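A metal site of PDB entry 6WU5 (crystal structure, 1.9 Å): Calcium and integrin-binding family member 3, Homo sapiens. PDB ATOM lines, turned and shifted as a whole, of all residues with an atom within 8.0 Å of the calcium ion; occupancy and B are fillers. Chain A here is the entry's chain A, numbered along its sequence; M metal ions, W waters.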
ATOM      1  N   PHE A 116     -10.424  22.788 -22.196  1.00  0.00           N
ATOM      2  CA  PHE A 116     -11.866  22.984 -22.295  1.00  0.00           C
ATOM      3  C   PHE A 116     -12.199  24.442 -22.557  1.00  0.00           C
ATOM      4  O   PHE A 116     -13.081  24.760 -23.356  1.00  0.00           O
ATOM      5  CB  PHE A 116     -12.547  22.487 -21.027  1.00  0.00           C
ATOM      6  CG  PHE A 116     -14.048  22.515 -21.077  1.00  0.00           C
ATOM      7  CD1 PHE A 116     -14.750  21.452 -21.616  1.00  0.00           C
ATOM      8  CD2 PHE A 116     -14.747  23.605 -20.592  1.00  0.00           C
ATOM      9  CE1 PHE A 116     -16.138  21.478 -21.669  1.00  0.00           C
ATOM     10  CE2 PHE A 116     -16.134  23.632 -20.628  1.00  0.00           C
ATOM     11  CZ  PHE A 116     -16.829  22.581 -21.167  1.00  0.00           C
ATOM     12  N   LYS A 117     -11.490  25.346 -21.892  1.00  0.00           N
ATOM     13  CA  LYS A 117     -11.758  26.772 -22.067  1.00  0.00           C
ATOM     14  C   LYS A 117     -11.449  27.234 -23.485  1.00  0.00           C
ATOM     15  O   LYS A 117     -12.215  28.025 -24.049  1.00  0.00           O
ATOM     16  CB  LYS A 117     -10.958  27.569 -21.038  1.00  0.00           C
ATOM     17  CG  LYS A 117     -11.591  27.526 -19.652  1.00  0.00           C
ATOM     18  CD  LYS A 117     -11.091  28.644 -18.748  1.00  0.00           C
ATOM     19  CE  LYS A 117     -12.020  28.839 -17.546  1.00  0.00           C
ATOM     20  NZ  LYS A 117     -13.437  29.154 -17.920  1.00  0.00           N
ATOM     21  N   TYR A 119     -11.459  25.368 -26.237  1.00  0.00           N
ATOM     22  CA  TYR A 119     -12.352  24.726 -27.188  1.00  0.00           C
ATOM     23  C   TYR A 119     -13.810  25.178 -27.032  1.00  0.00           C
ATOM     24  O   TYR A 119     -14.615  24.910 -27.931  1.00  0.00           O
ATOM     25  CB  TYR A 119     -12.271  23.194 -27.059  1.00  0.00           C
ATOM     26  CG  TYR A 119     -10.858  22.654 -27.201  1.00  0.00           C
ATOM     27  CD1 TYR A 119      -9.929  23.280 -28.022  1.00  0.00           C
ATOM     28  CD2 TYR A 119     -10.458  21.516 -26.506  1.00  0.00           C
ATOM     29  CE1 TYR A 119      -8.641  22.802 -28.142  1.00  0.00           C
ATOM     30  CE2 TYR A 119      -9.170  21.021 -26.637  1.00  0.00           C
ATOM     31  CZ  TYR A 119      -8.269  21.672 -27.458  1.00  0.00           C
ATOM     32  OH  TYR A 119      -6.974  21.205 -27.580  1.00  0.00           O
ATOM     33  N   ASP A 120     -14.150  25.845 -25.930  1.00  0.00           N
ATOM     34  CA  ASP A 120     -15.513  26.367 -25.724  1.00  0.00           C
ATOM     35  C   ASP A 120     -15.574  27.752 -26.364  1.00  0.00           C
ATOM     36  O   ASP A 120     -15.456  28.791 -25.711  1.00  0.00           O
ATOM     37  CB  ASP A 120     -15.830  26.390 -24.235  1.00  0.00           C
ATOM     38  CG  ASP A 120     -17.062  27.234 -23.910  1.00  0.00           C
ATOM     39  OD1 ASP A 120     -17.971  27.364 -24.765  1.00  0.00           O
ATOM     40  OD2 ASP A 120     -17.144  27.754 -22.775  1.00  0.00           O
ATOM     41  N   PHE A 121     -15.775  27.752 -27.685  1.00  0.00           N
ATOM     42  CA  PHE A 121     -15.623  28.996 -28.454  1.00  0.00           C
ATOM     43  C   PHE A 121     -16.621  30.063 -28.029  1.00  0.00           C
ATOM     44  O   PHE A 121     -16.257  31.219 -27.836  1.00  0.00           O
ATOM     45  CB  PHE A 121     -15.744  28.692 -29.952  1.00  0.00           C
ATOM     46  CG  PHE A 121     -14.652  27.785 -30.454  1.00  0.00           C
ATOM     47  CD1 PHE A 121     -13.355  28.259 -30.544  1.00  0.00           C
ATOM     48  CD2 PHE A 121     -14.916  26.481 -30.795  1.00  0.00           C
ATOM     49  CE1 PHE A 121     -12.345  27.432 -30.980  1.00  0.00           C
ATOM     50  CE2 PHE A 121     -13.892  25.646 -31.237  1.00  0.00           C
ATOM     51  CZ  PHE A 121     -12.609  26.128 -31.321  1.00  0.00           C
ATOM     52  N   ASN A 122     -17.899  29.700 -27.872  1.00  0.00           N
ATOM     53  CA  ASN A 122     -18.893  30.702 -27.495  1.00  0.00           C
ATOM     54  C   ASN A 122     -18.936  30.965 -25.996  1.00  0.00           C
ATOM     55  O   ASN A 122     -19.835  31.677 -25.531  1.00  0.00           O
ATOM     56  CB  ASN A 122     -20.280  30.299 -27.999  1.00  0.00           C
ATOM     57  CG  ASN A 122     -20.730  28.958 -27.476  1.00  0.00           C
ATOM     58  OD1 ASN A 122     -19.998  27.975 -27.558  1.00  0.00           O
ATOM     59  ND2 ASN A 122     -21.942  28.913 -26.921  1.00  0.00           N
ATOM     60  N   ASN A 123     -17.975  30.430 -25.230  1.00  0.00           N
ATOM     61  CA  ASN A 123     -17.806  30.773 -23.817  1.00  0.00           C
ATOM     62  C   ASN A 123     -19.080  30.554 -23.010  1.00  0.00           C
ATOM     63  O   ASN A 123     -19.423  31.352 -22.143  1.00  0.00           O
ATOM     64  CB  ASN A 123     -17.330  32.222 -23.670  1.00  0.00           C
ATOM     65  CG  ASN A 123     -15.915  32.440 -24.156  1.00  0.00           C
ATOM     66  OD1 ASN A 123     -15.003  31.701 -23.786  1.00  0.00           O
ATOM     67  ND2 ASN A 123     -15.728  33.457 -24.997  1.00  0.00           N
ATOM     68  N   ASP A 124     -19.798  29.465 -23.291  1.00  0.00           N
ATOM     69  CA  ASP A 124     -20.990  29.136 -22.520  1.00  0.00           C
ATOM     70  C   ASP A 124     -20.790  27.940 -21.601  1.00  0.00           C
ATOM     71  O   ASP A 124     -21.781  27.400 -21.092  1.00  0.00           O
ATOM     72  CB  ASP A 124     -22.185  28.910 -23.464  1.00  0.00           C
ATOM     73  CG  ASP A 124     -22.071  27.628 -24.250  1.00  0.00           C
ATOM     74  OD1 ASP A 124     -20.995  27.008 -24.240  1.00  0.00           O
ATOM     75  OD2 ASP A 124     -23.071  27.259 -24.911  1.00  0.00           O
ATOM     76  N   ASP A 125     -19.549  27.538 -21.361  1.00  0.00           N
ATOM     77  CA  ASP A 125     -19.191  26.453 -20.443  1.00  0.00           C
ATOM     78  C   ASP A 125     -19.596  25.086 -20.961  1.00  0.00           C
ATOM     79  O   ASP A 125     -19.713  24.129 -20.184  1.00  0.00           O
ATOM     80  CB  ASP A 125     -19.797  26.691 -19.060  1.00  0.00           C
ATOM     81  CG  ASP A 125     -19.376  28.015 -18.452  1.00  0.00           C
ATOM     82  OD1 ASP A 125     -18.176  28.347 -18.553  1.00  0.00           O
ATOM     83  OD2 ASP A 125     -20.231  28.733 -17.885  1.00  0.00           O
ATOM     84  N   TYR A 126     -19.821  24.962 -22.267  1.00  0.00           N
ATOM     85  CA  TYR A 126     -20.064  23.685 -22.906  1.00  0.00           C
ATOM     86  C   TYR A 126     -19.233  23.609 -24.184  1.00  0.00           C
ATOM     87  O   TYR A 126     -18.977  24.634 -24.830  1.00  0.00           O
ATOM     88  CB  TYR A 126     -21.549  23.479 -23.264  1.00  0.00           C
ATOM     89  CG  TYR A 126     -22.465  23.324 -22.084  1.00  0.00           C
ATOM     90  CD1 TYR A 126     -22.526  22.119 -21.384  1.00  0.00           C
ATOM     91  CD2 TYR A 126     -23.280  24.362 -21.662  1.00  0.00           C
ATOM     92  CE1 TYR A 126     -23.381  21.969 -20.292  1.00  0.00           C
ATOM     93  CE2 TYR A 126     -24.121  24.220 -20.582  1.00  0.00           C
ATOM     94  CZ  TYR A 126     -24.175  23.025 -19.900  1.00  0.00           C
ATOM     95  OH  TYR A 126     -25.015  22.882 -18.821  1.00  0.00           O
ATOM     96  N   ILE A 127     -18.824  22.399 -24.549  1.00  0.00           N
ATOM     97  CA  ILE A 127     -18.338  22.130 -25.891  1.00  0.00           C
ATOM     98  C   ILE A 127     -19.510  21.516 -26.640  1.00  0.00           C
ATOM     99  O   ILE A 127     -19.905  20.370 -26.364  1.00  0.00           O
ATOM    100  CB  ILE A 127     -17.115  21.195 -25.891  1.00  0.00           C
ATOM    101  CG1 ILE A 127     -15.896  21.899 -25.294  1.00  0.00           C
ATOM    102  CG2 ILE A 127     -16.806  20.735 -27.314  1.00  0.00           C
ATOM    103  CD1 ILE A 127     -14.716  20.953 -25.061  1.00  0.00           C
ATOM    104  N   CYS A 128     -20.115  22.272 -27.541  1.00  0.00           N
ATOM    105  CA  CYS A 128     -21.227  21.778 -28.317  1.00  0.00           C
ATOM    106  C   CYS A 128     -20.715  21.068 -29.571  1.00  0.00           C
ATOM    107  O   CYS A 128     -19.513  21.003 -29.829  1.00  0.00           O
ATOM    108  CB  CYS A 128     -22.179  22.915 -28.668  1.00  0.00           C
ATOM    109  SG  CYS A 128     -21.537  24.072 -29.884  1.00  0.00           S
ATOM    110  N   ALA A 129     -21.645  20.519 -30.366  1.00  0.00           N
ATOM    111  CA  ALA A 129     -21.223  19.795 -31.553  1.00  0.00           C
ATOM    112  C   ALA A 129     -20.439  20.698 -32.493  1.00  0.00           C
ATOM    113  O   ALA A 129     -19.496  20.242 -33.151  1.00  0.00           O
ATOM    114  CB  ALA A 129     -22.435  19.201 -32.273  1.00  0.00           C
ATOM    115  N   TRP A 130     -20.794  21.977 -32.574  1.00  0.00           N
ATOM    116  CA  TRP A 130     -20.087  22.881 -33.473  1.00  0.00           C
ATOM    117  C   TRP A 130     -18.707  23.227 -32.913  1.00  0.00           C
ATOM    118  O   TRP A 130     -17.713  23.222 -33.661  1.00  0.00           O
ATOM    119  CB  TRP A 130     -20.933  24.131 -33.707  1.00  0.00           C
ATOM    120  CG  TRP A 130     -20.315  25.172 -34.595  1.00  0.00           C
ATOM    121  CD1 TRP A 130     -20.179  26.499 -34.322  1.00  0.00           C
ATOM    122  CD2 TRP A 130     -19.771  24.984 -35.922  1.00  0.00           C
ATOM    123  NE1 TRP A 130     -19.580  27.156 -35.368  1.00  0.00           N
ATOM    124  CE2 TRP A 130     -19.320  26.249 -36.358  1.00  0.00           C
ATOM    125  CE3 TRP A 130     -19.618  23.882 -36.757  1.00  0.00           C
ATOM    126  CZ2 TRP A 130     -18.724  26.426 -37.613  1.00  0.00           C
ATOM    127  CZ3 TRP A 130     -19.028  24.063 -38.001  1.00  0.00           C
ATOM    128  CH2 TRP A 130     -18.591  25.338 -38.414  1.00  0.00           C
ATOM    129  N   ASP A 131     -18.613  23.505 -31.620  1.00  0.00           N
ATOM    130  CA  ASP A 131     -17.307  23.646 -30.969  1.00  0.00           C
ATOM    131  C   ASP A 131     -16.456  22.397 -31.180  1.00  0.00           C
ATOM    132  O   ASP A 131     -15.266  22.468 -31.488  1.00  0.00           O
ATOM    133  CB  ASP A 131     -17.457  23.882 -29.476  1.00  0.00           C
ATOM    134  CG  ASP A 131     -18.011  25.244 -29.141  1.00  0.00           C
ATOM    135  OD1 ASP A 131     -17.947  26.145 -29.994  1.00  0.00           O
ATOM    136  OD2 ASP A 131     -18.519  25.392 -28.022  1.00  0.00           O
ATOM    137  N   LEU A 132     -17.058  21.231 -30.955  1.00  0.00           N
ATOM    138  CA  LEU A 132     -16.312  19.985 -31.089  1.00  0.00           C
ATOM    139  C   LEU A 132     -15.834  19.779 -32.517  1.00  0.00           C
ATOM    140  O   LEU A 132     -14.673  19.426 -32.759  1.00  0.00           O
ATOM    141  CB  LEU A 132     -17.177  18.816 -30.631  1.00  0.00           C
ATOM    142  CG  LEU A 132     -16.509  17.443 -30.685  1.00  0.00           C
ATOM    143  CD1 LEU A 132     -15.216  17.464 -29.891  1.00  0.00           C
ATOM    144  CD2 LEU A 132     -17.442  16.353 -30.179  1.00  0.00           C
ATOM    145  N   ARG A 167     -24.085  18.081 -25.899  1.00  0.00           N
ATOM    146  CA  ARG A 167     -22.881  18.876 -25.702  1.00  0.00           C
ATOM    147  C   ARG A 167     -22.081  18.306 -24.542  1.00  0.00           C
ATOM    148  O   ARG A 167     -22.596  17.528 -23.727  1.00  0.00           O
ATOM    149  CB  ARG A 167     -23.230  20.344 -25.478  1.00  0.00           C
ATOM    150  CG  ARG A 167     -24.283  20.553 -24.407  1.00  0.00           C
ATOM    151  CD  ARG A 167     -24.889  21.937 -24.472  1.00  0.00           C
ATOM    152  NE  ARG A 167     -25.863  22.133 -23.401  1.00  0.00           N
ATOM    153  CZ  ARG A 167     -26.322  23.309 -22.998  1.00  0.00           C
ATOM    154  NH1 ARG A 167     -25.900  24.421 -23.585  1.00  0.00           N
ATOM    155  NH2 ARG A 167     -27.210  23.369 -22.018  1.00  0.00           N
ATOM    156  N   LEU A 168     -20.818  18.706 -24.469  1.00  0.00           N
ATOM    157  CA  LEU A 168     -19.899  18.219 -23.451  1.00  0.00           C
ATOM    158  C   LEU A 168     -19.700  19.262 -22.365  1.00  0.00           C
ATOM    159  O   LEU A 168     -19.355  20.405 -22.652  1.00  0.00           O
ATOM    160  CB  LEU A 168     -18.542  17.880 -24.058  1.00  0.00           C
ATOM    161  CG  LEU A 168     -18.479  16.857 -25.191  1.00  0.00           C
ATOM    162  CD1 LEU A 168     -17.034  16.785 -25.646  1.00  0.00           C
ATOM    163  CD2 LEU A 168     -18.995  15.506 -24.764  1.00  0.00           C
HETATM  164 CA    CA M   1     -19.612  26.423 -26.179  1.00  0.00          CA
HETATM  165  O   HOH W   1     -21.657  25.650 -27.248  1.00  0.00           O
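The backbone NH (N) of Asn 123 lies close to the side-chain carboxylate (OD1) of Asp 120.
The side-chain carboxylate of Asp 120 sits at hydrogen-bond distance from the backbone NH of Asp 125 (2.8 Å).
The backbone NH (N) of Asp 131 lies within hydrogen-bond range of the side-chain sulfur (SG) of Cys 128, at 3.4 Å.
The calcium ion is bound by the side-chain amide oxygen (OD1) of Asn 122 (2.1 Å), the backbone carbonyl oxygen (O) of Tyr 126 (2.3 Å), the side-chain carboxylate (OD1) of Asp 120 (2.4 Å), the side-chain carboxylate (OD2) of Asp 131 (2.4 Å), water W1 (2.4 Å) and the side-chain carboxylate (OD1) of Asp 124 (2.5 Å).
The calcium ion has six donor atoms within binding distance.
Water W1 lies within hydrogen-bond range of the side-chain sulfur (SG) of Cys 128 (3.1 Å), the side-chain carboxylate (OD2) of Asp 124 (3.2 Å) and the side-chain amide nitrogen (ND2) of Asn 122 (3.3 Å).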
